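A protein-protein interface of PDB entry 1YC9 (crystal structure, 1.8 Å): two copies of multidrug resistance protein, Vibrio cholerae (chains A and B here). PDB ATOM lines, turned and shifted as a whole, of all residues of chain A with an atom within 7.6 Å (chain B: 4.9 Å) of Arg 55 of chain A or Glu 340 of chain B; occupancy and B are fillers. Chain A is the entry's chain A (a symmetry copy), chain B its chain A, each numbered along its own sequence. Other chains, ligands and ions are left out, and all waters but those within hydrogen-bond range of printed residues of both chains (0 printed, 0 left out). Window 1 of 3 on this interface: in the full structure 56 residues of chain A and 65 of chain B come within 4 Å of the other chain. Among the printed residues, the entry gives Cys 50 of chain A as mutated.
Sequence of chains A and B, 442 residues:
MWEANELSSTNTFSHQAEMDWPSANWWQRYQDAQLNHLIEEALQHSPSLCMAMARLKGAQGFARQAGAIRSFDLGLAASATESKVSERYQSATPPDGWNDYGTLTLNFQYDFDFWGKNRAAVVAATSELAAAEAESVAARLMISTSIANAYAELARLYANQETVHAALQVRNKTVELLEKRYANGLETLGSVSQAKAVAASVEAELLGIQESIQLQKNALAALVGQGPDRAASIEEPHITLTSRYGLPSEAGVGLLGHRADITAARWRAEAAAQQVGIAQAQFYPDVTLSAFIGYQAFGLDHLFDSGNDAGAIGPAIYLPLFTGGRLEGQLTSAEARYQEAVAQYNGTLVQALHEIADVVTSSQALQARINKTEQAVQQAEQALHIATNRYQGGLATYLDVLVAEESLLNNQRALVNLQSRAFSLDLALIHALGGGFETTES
Among the printed residues, pairs that only touch across the chains: Pro 47 of chain A with Ala 343 of chain B, Cys 50 of chain A with Ala 343 of chain B, Met 51 of chain A with Ala 343 of chain B, Met 51 of chain A with Gln 344 of chain B, Ala 54 of chain A with Ala 336 of chain B, Ala 54 of chain A with Glu 340 of chain B, Arg 55 of chain A with Glu 340 of chain B, Lys 57 of chain A with Ala 336 of chain B and Gly 58 of chain A with Ala 336 of chain B.
No position is printed for both chains. Of the 10 pairs that touch across the chains among the printed residues, none has its exchanged pair printed and touching as well.
Arg 55 of chain A touches just one residue of chain B: Glu 340. Glu 340 of chain B touches two residues of chain A. Of the printed residues of chain A, Ala 336 of chain B touches Ala 54 (3.4 Å), Lys 57 (3.9 Å) and Gly 58 (3.5 Å). Of the printed residues of chain B, Ala 54 of chain A touches Ala 336 (3.4 Å) and Glu 340 (3.5 Å). Of the printed residues of chain B, Gly 58 of chain A touches Ala 336. Ala 132 of chain A touches none of the printed residues of chain B. The nearest residue of chain A that does not touch Glu 340 of chain B is Met 51 of chain A (4.2 Å).
Of the 20 printed residues of chain A, 7 touch a printed residue of chain B. Hydrophobic or aromatic side chains of chain A within 4 Å of the printed part of chain B: Pro 47, Met 51 and Ala 54. Along chain A the printed residues that touch a printed residue of chain B span positions 47 to 58. Hydrophobic or aromatic side chains of chain B that line the printed part of chain A: Ala 336 and Ala 343. Among the printed residues, 10 pairs touch across the chains.
NZ of Lys 57 of chain A lies close to NE2 of Gln 339 of chain B, 2.9 Å away.
The side-chain carboxylate of Glu 340 of chain B lies within salt-bridge range of the guanidinium group of Arg 337 of chain B (2.8 Å). NH1 of Arg 337 of chain B sits at hydrogen-bond distance from OE1 of Gln 344 of chain B (2.9 Å).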
ATOM      1  N   PRO A  47       9.831   3.609  14.456  1.00  0.00           N
ATOM      2  CA  PRO A  47      10.640   2.583  15.125  1.00  0.00           C
ATOM      3  C   PRO A  47      12.163   2.703  14.934  1.00  0.00           C
ATOM      4  O   PRO A  47      12.885   2.496  15.880  1.00  0.00           O
ATOM      5  CB  PRO A  47      10.089   1.274  14.541  1.00  0.00           C
ATOM      6  CG  PRO A  47       8.659   1.621  14.189  1.00  0.00           C
ATOM      7  CD  PRO A  47       8.758   3.015  13.627  1.00  0.00           C
ATOM      8  N   LEU A  49      13.837   5.410  14.434  1.00  0.00           N
ATOM      9  CA  LEU A  49      14.180   6.523  15.294  1.00  0.00           C
ATOM     10  C   LEU A  49      14.311   6.061  16.738  1.00  0.00           C
ATOM     11  O   LEU A  49      15.316   6.288  17.377  1.00  0.00           O
ATOM     12  CB  LEU A  49      13.127   7.623  15.218  1.00  0.00           C
ATOM     13  CG  LEU A  49      13.385   8.734  16.229  1.00  0.00           C
ATOM     14  CD1 LEU A  49      14.611   9.517  15.845  1.00  0.00           C
ATOM     15  CD2 LEU A  49      12.207   9.637  16.445  1.00  0.00           C
ATOM     16  N   CYS A  50      13.271   5.417  17.241  1.00  0.00           N
ATOM     17  CA  CYS A  50      13.238   5.027  18.633  1.00  0.00           C
ATOM     18  C   CYS A  50      14.347   4.061  19.006  1.00  0.00           C
ATOM     19  O   CYS A  50      14.886   4.156  20.090  1.00  0.00           O
ATOM     20  CB  CYS A  50      11.862   4.508  19.052  1.00  0.00           C
ATOM     21  SG  CYS A  50      10.528   5.694  18.784  1.00  0.00           S
ATOM     22  N   MET A  51      14.697   3.151  18.102  1.00  0.00           N
ATOM     23  CA  MET A  51      15.744   2.193  18.373  1.00  0.00           C
ATOM     24  C   MET A  51      17.068   2.940  18.488  1.00  0.00           C
ATOM     25  O   MET A  51      17.885   2.624  19.320  1.00  0.00           O
ATOM     26  CB  MET A  51      15.852   1.179  17.257  1.00  0.00           C
ATOM     27  CG  MET A  51      14.721   0.166  17.260  1.00  0.00           C
ATOM     28  SD  MET A  51      14.838  -1.072  15.986  1.00  0.00           S
ATOM     29  CE  MET A  51      16.565  -1.503  16.107  1.00  0.00           C
ATOM     30  N   ALA A  52      17.290   3.900  17.596  1.00  0.00           N
ATOM     31  CA  ALA A  52      18.489   4.707  17.647  1.00  0.00           C
ATOM     32  C   ALA A  52      18.615   5.515  18.974  1.00  0.00           C
ATOM     33  O   ALA A  52      19.706   5.545  19.570  1.00  0.00           O
ATOM     34  CB  ALA A  52      18.544   5.654  16.429  1.00  0.00           C
ATOM     35  N   MET A  53      17.530   6.153  19.400  1.00  0.00           N
ATOM     36  CA  MET A  53      17.416   6.872  20.672  1.00  0.00           C
ATOM     37  C   MET A  53      17.770   5.931  21.828  1.00  0.00           C
ATOM     38  O   MET A  53      18.512   6.263  22.735  1.00  0.00           O
ATOM     39  CB  MET A  53      15.969   7.392  20.895  1.00  0.00           C
ATOM     40  CG  MET A  53      15.518   8.511  19.916  1.00  0.00           C
ATOM     41  SD  MET A  53      13.955   9.371  20.206  1.00  0.00           S
ATOM     42  CE  MET A  53      12.624   8.153  20.056  1.00  0.00           C
ATOM     43  N   ALA A  54      17.205   4.732  21.770  1.00  0.00           N
ATOM     44  CA  ALA A  54      17.380   3.721  22.815  1.00  0.00           C
ATOM     45  C   ALA A  54      18.820   3.247  22.924  1.00  0.00           C
ATOM     46  O   ALA A  54      19.359   3.125  24.027  1.00  0.00           O
ATOM     47  CB  ALA A  54      16.456   2.549  22.574  1.00  0.00           C
ATOM     48  N   ARG A  55      19.447   3.021  21.775  1.00  0.00           N
ATOM     49  CA  ARG A  55      20.844   2.609  21.726  1.00  0.00           C
ATOM     50  C   ARG A  55      21.806   3.683  22.232  1.00  0.00           C
ATOM     51  O   ARG A  55      22.886   3.366  22.732  1.00  0.00           O
ATOM     52  CB  ARG A  55      21.227   2.178  20.309  1.00  0.00           C
ATOM     53  CG  ARG A  55      20.529   0.912  19.838  1.00  0.00           C
ATOM     54  N   LEU A  56      21.421   4.951  22.104  1.00  0.00           N
ATOM     55  CA  LEU A  56      22.217   6.027  22.667  1.00  0.00           C
ATOM     56  C   LEU A  56      22.012   6.048  24.185  1.00  0.00           C
ATOM     57  O   LEU A  56      22.964   6.139  24.942  1.00  0.00           O
ATOM     58  CB  LEU A  56      21.869   7.381  22.005  1.00  0.00           C
ATOM     59  CG  LEU A  56      22.525   8.595  22.660  1.00  0.00           C
ATOM     60  CD1 LEU A  56      24.045   8.443  22.662  1.00  0.00           C
ATOM     61  CD2 LEU A  56      22.098   9.833  21.889  1.00  0.00           C
ATOM     62  N   LYS A  57      20.769   5.947  24.643  1.00  0.00           N
ATOM     63  CA  LYS A  57      20.492   5.944  26.062  1.00  0.00           C
ATOM     64  C   LYS A  57      21.221   4.781  26.735  1.00  0.00           C
ATOM     65  O   LYS A  57      21.732   4.923  27.841  1.00  0.00           O
ATOM     66  CB  LYS A  57      18.984   5.925  26.335  1.00  0.00           C
ATOM     67  CG  LYS A  57      18.575   5.938  27.791  1.00  0.00           C
ATOM     68  CD  LYS A  57      17.068   5.916  27.961  1.00  0.00           C
ATOM     69  CE  LYS A  57      16.703   5.824  29.420  1.00  0.00           C
ATOM     70  NZ  LYS A  57      15.254   5.969  29.688  1.00  0.00           N
ATOM     71  N   GLY A  58      21.315   3.660  26.045  1.00  0.00           N
ATOM     72  CA  GLY A  58      22.026   2.497  26.550  1.00  0.00           C
ATOM     73  C   GLY A  58      23.465   2.817  26.839  1.00  0.00           C
ATOM     74  O   GLY A  58      23.999   2.491  27.897  1.00  0.00           O
ATOM     75  N   ALA A  59      24.107   3.431  25.866  1.00  0.00           N
ATOM     76  CA  ALA A  59      25.514   3.803  26.004  1.00  0.00           C
ATOM     77  C   ALA A  59      25.693   4.819  27.153  1.00  0.00           C
ATOM     78  O   ALA A  59      26.705   4.800  27.851  1.00  0.00           O
ATOM     79  CB  ALA A  59      26.028   4.392  24.712  1.00  0.00           C
ATOM     80  N   GLN A  60      24.709   5.694  27.335  1.00  0.00           N
ATOM     81  CA  GLN A  60      24.713   6.636  28.443  1.00  0.00           C
ATOM     82  C   GLN A  60      24.680   5.906  29.779  1.00  0.00           C
ATOM     83  O   GLN A  60      25.449   6.185  30.692  1.00  0.00           O
ATOM     84  CB  GLN A  60      23.561   7.655  28.325  1.00  0.00           C
ATOM     85  CG  GLN A  60      23.723   8.649  27.131  1.00  0.00           C
ATOM     86  CD  GLN A  60      22.445   9.433  26.833  1.00  0.00           C
ATOM     87  OE1 GLN A  60      21.404   9.080  27.329  1.00  0.00           O
ATOM     88  NE2 GLN A  60      22.544  10.475  26.001  1.00  0.00           N
ATOM     89  N   GLY A  61      23.753   4.958  29.910  1.00  0.00           N
ATOM     90  CA  GLY A  61      23.718   4.109  31.086  1.00  0.00           C
ATOM     91  C   GLY A  61      24.968   3.316  31.314  1.00  0.00           C
ATOM     92  O   GLY A  61      25.385   3.162  32.464  1.00  0.00           O
ATOM     93  N   GLU A 128      33.362   5.110  24.271  1.00  0.00           N
ATOM     94  CA  GLU A 128      32.252   4.364  23.701  1.00  0.00           C
ATOM     95  C   GLU A 128      31.008   5.194  23.613  1.00  0.00           C
ATOM     96  O   GLU A 128      30.239   5.119  22.656  1.00  0.00           O
ATOM     97  CB  GLU A 128      31.922   3.079  24.493  1.00  0.00           C
ATOM     98  CG  GLU A 128      33.044   2.059  24.306  1.00  0.00           C
ATOM     99  CD  GLU A 128      33.089   1.380  22.929  1.00  0.00           C
ATOM    100  OE1 GLU A 128      32.190   1.651  22.046  1.00  0.00           O
ATOM    101  OE2 GLU A 128      34.059   0.558  22.741  1.00  0.00           O
ATOM    102  N   LEU A 129      30.815   6.017  24.614  1.00  0.00           N
ATOM    103  CA  LEU A 129      29.648   6.904  24.548  1.00  0.00           C
ATOM    104  C   LEU A 129      29.794   7.898  23.395  1.00  0.00           C
ATOM    105  O   LEU A 129      28.848   8.187  22.681  1.00  0.00           O
ATOM    106  CB  LEU A 129      29.457   7.612  25.884  1.00  0.00           C
ATOM    107  CG  LEU A 129      28.352   8.680  25.909  1.00  0.00           C
ATOM    108  CD1 LEU A 129      27.019   8.062  25.514  1.00  0.00           C
ATOM    109  CD2 LEU A 129      28.262   9.324  27.287  1.00  0.00           C
ATOM    110  N   ALA A 132      28.899   6.152  20.434  1.00  0.00           N
ATOM    111  CA  ALA A 132      27.441   6.008  20.396  1.00  0.00           C
ATOM    112  C   ALA A 132      26.704   7.295  19.969  1.00  0.00           C
ATOM    113  O   ALA A 132      25.670   7.273  19.248  1.00  0.00           O
ATOM    114  CB  ALA A 132      26.939   5.516  21.680  1.00  0.00           C
ATOM    115  N   GLU A 133      27.255   8.415  20.393  1.00  0.00           N
ATOM    116  CA  GLU A 133      26.703   9.719  19.994  1.00  0.00           C
ATOM    117  C   GLU A 133      26.826   9.898  18.476  1.00  0.00           C
ATOM    118  O   GLU A 133      25.870  10.276  17.800  1.00  0.00           O
ATOM    119  CB  GLU A 133      27.383  10.835  20.767  1.00  0.00           C
ATOM    120  CG  GLU A 133      26.979  10.891  22.212  1.00  0.00           C
ATOM    121  CD  GLU A 133      27.776  11.883  23.050  1.00  0.00           C
ATOM    122  OE1 GLU A 133      28.755  12.432  22.524  1.00  0.00           O
ATOM    123  OE2 GLU A 133      27.412  12.078  24.236  1.00  0.00           O
ATOM    124  N   GLU A 135      27.136   7.458  16.338  1.00  0.00           N
ATOM    125  CA  GLU A 135      26.282   6.499  15.677  1.00  0.00           C
ATOM    126  C   GLU A 135      24.821   6.960  15.650  1.00  0.00           C
ATOM    127  O   GLU A 135      24.118   6.662  14.698  1.00  0.00           O
ATOM    128  CB  GLU A 135      26.424   5.121  16.296  1.00  0.00           C
ATOM    129  CG  GLU A 135      27.783   4.535  15.950  1.00  0.00           C
ATOM    130  CD  GLU A 135      27.993   3.154  16.502  1.00  0.00           C
ATOM    131  OE1 GLU A 135      27.343   2.804  17.498  1.00  0.00           O
ATOM    132  OE2 GLU A 135      28.832   2.404  15.929  1.00  0.00           O
ATOM    133  N   SER A 136      24.386   7.722  16.641  1.00  0.00           N
ATOM    134  CA  SER A 136      23.033   8.281  16.622  1.00  0.00           C
ATOM    135  C   SER A 136      22.860   9.274  15.457  1.00  0.00           C
ATOM    136  O   SER A 136      21.804   9.321  14.835  1.00  0.00           O
ATOM    137  CB  SER A 136      22.626   8.925  17.955  1.00  0.00           C
ATOM    138  OG  SER A 136      23.360  10.083  18.200  1.00  0.00           O
ATOM    139  N   ALA B 336      16.574   1.651  28.554  1.00  0.00           N
ATOM    140  CA  ALA B 336      16.965   1.732  27.171  1.00  0.00           C
ATOM    141  C   ALA B 336      16.688   0.415  26.422  1.00  0.00           C
ATOM    142  O   ALA B 336      16.214   0.426  25.297  1.00  0.00           O
ATOM    143  CB  ALA B 336      18.376   2.061  27.066  1.00  0.00           C
ATOM    144  N   ARG B 337      17.002  -0.693  27.051  1.00  0.00           N
ATOM    145  CA  ARG B 337      16.736  -1.982  26.428  1.00  0.00           C
ATOM    146  C   ARG B 337      15.222  -2.158  26.245  1.00  0.00           C
ATOM    147  O   ARG B 337      14.806  -2.647  25.183  1.00  0.00           O
ATOM    148  CB  ARG B 337      17.345  -3.135  27.237  1.00  0.00           C
ATOM    149  CG  ARG B 337      16.893  -4.501  26.786  1.00  0.00           C
ATOM    150  CD  ARG B 337      17.203  -4.848  25.314  1.00  0.00           C
ATOM    151  NE  ARG B 337      16.462  -6.043  24.890  1.00  0.00           N
ATOM    152  CZ  ARG B 337      15.892  -6.244  23.679  1.00  0.00           C
ATOM    153  NH1 ARG B 337      16.045  -5.386  22.664  1.00  0.00           N
ATOM    154  NH2 ARG B 337      15.255  -7.411  23.448  1.00  0.00           N
ATOM    155  N   TYR B 338      14.417  -1.763  27.230  1.00  0.00           N
ATOM    156  CA  TYR B 338      12.950  -1.824  27.079  1.00  0.00           C
ATOM    157  C   TYR B 338      12.457  -1.001  25.919  1.00  0.00           C
ATOM    158  O   TYR B 338      11.639  -1.435  25.112  1.00  0.00           O
ATOM    159  CB  TYR B 338      12.245  -1.404  28.344  1.00  0.00           C
ATOM    160  CG  TYR B 338      10.771  -1.349  28.198  1.00  0.00           C
ATOM    161  CD1 TYR B 338      10.106  -0.155  28.257  1.00  0.00           C
ATOM    162  CD2 TYR B 338      10.030  -2.517  27.973  1.00  0.00           C
ATOM    163  CE1 TYR B 338       8.757  -0.082  28.108  1.00  0.00           C
ATOM    164  CE2 TYR B 338       8.670  -2.447  27.802  1.00  0.00           C
ATOM    165  CZ  TYR B 338       8.032  -1.238  27.882  1.00  0.00           C
ATOM    166  OH  TYR B 338       6.664  -1.154  27.725  1.00  0.00           O
ATOM    167  N   GLN B 339      12.960   0.225  25.834  1.00  0.00           N
ATOM    168  CA  GLN B 339      12.583   1.125  24.766  1.00  0.00           C
ATOM    169  C   GLN B 339      12.970   0.566  23.402  1.00  0.00           C
ATOM    170  O   GLN B 339      12.180   0.665  22.452  1.00  0.00           O
ATOM    171  CB  GLN B 339      13.206   2.512  25.041  1.00  0.00           C
ATOM    172  CG  GLN B 339      12.556   3.199  26.207  1.00  0.00           C
ATOM    173  CD  GLN B 339      13.229   4.532  26.593  1.00  0.00           C
ATOM    174  OE1 GLN B 339      12.829   5.600  26.119  1.00  0.00           O
ATOM    175  NE2 GLN B 339      14.167   4.472  27.484  1.00  0.00           N
ATOM    176  N   GLU B 340      14.165  -0.008  23.296  1.00  0.00           N
ATOM    177  CA  GLU B 340      14.625  -0.650  22.118  1.00  0.00           C
ATOM    178  C   GLU B 340      13.689  -1.806  21.740  1.00  0.00           C
ATOM    179  O   GLU B 340      13.302  -1.943  20.576  1.00  0.00           O
ATOM    180  CB  GLU B 340      15.994  -1.203  22.327  1.00  0.00           C
ATOM    181  CG  GLU B 340      16.535  -1.910  21.117  1.00  0.00           C
ATOM    182  CD  GLU B 340      17.848  -2.558  21.379  1.00  0.00           C
ATOM    183  OE1 GLU B 340      17.961  -3.326  22.381  1.00  0.00           O
ATOM    184  OE2 GLU B 340      18.754  -2.310  20.582  1.00  0.00           O
ATOM    185  N   ALA B 341      13.374  -2.629  22.725  1.00  0.00           N
ATOM    186  CA  ALA B 341      12.522  -3.808  22.468  1.00  0.00           C
ATOM    187  C   ALA B 341      11.113  -3.413  22.003  1.00  0.00           C
ATOM    188  O   ALA B 341      10.524  -4.086  21.117  1.00  0.00           O
ATOM    189  CB  ALA B 341      12.488  -4.694  23.690  1.00  0.00           C
ATOM    190  N   VAL B 342      10.572  -2.327  22.539  1.00  0.00           N
ATOM    191  CA  VAL B 342       9.255  -1.821  22.140  1.00  0.00           C
ATOM    192  C   VAL B 342       9.350  -1.309  20.696  1.00  0.00           C
ATOM    193  O   VAL B 342       8.449  -1.527  19.878  1.00  0.00           O
ATOM    194  CB  VAL B 342       8.753  -0.723  23.091  1.00  0.00           C
ATOM    195  CG1 VAL B 342       7.593   0.063  22.528  1.00  0.00           C
ATOM    196  CG2 VAL B 342       8.401  -1.288  24.417  1.00  0.00           C
ATOM    197  N   ALA B 343      10.452  -0.631  20.391  1.00  0.00           N
ATOM    198  CA  ALA B 343      10.640  -0.096  19.060  1.00  0.00           C
ATOM    199  C   ALA B 343      10.800  -1.242  18.086  1.00  0.00           C
ATOM    200  O   ALA B 343      10.276  -1.172  16.958  1.00  0.00           O
ATOM    201  CB  ALA B 343      11.871   0.833  18.999  1.00  0.00           C
ATOM    202  N   GLN B 344      11.518  -2.287  18.511  1.00  0.00           N
ATOM    203  CA  GLN B 344      11.683  -3.474  17.707  1.00  0.00           C
ATOM    204  C   GLN B 344      10.330  -4.140  17.409  1.00  0.00           C
ATOM    205  O   GLN B 344      10.091  -4.561  16.269  1.00  0.00           O
ATOM    206  CB  GLN B 344      12.670  -4.451  18.305  1.00  0.00           C
ATOM    207  CG  GLN B 344      14.122  -4.033  18.128  1.00  0.00           C
ATOM    208  CD  GLN B 344      15.088  -4.862  18.974  1.00  0.00           C
ATOM    209  OE1 GLN B 344      14.737  -5.287  20.080  1.00  0.00           O
ATOM    210  NE2 GLN B 344      16.329  -5.038  18.487  1.00  0.00           N
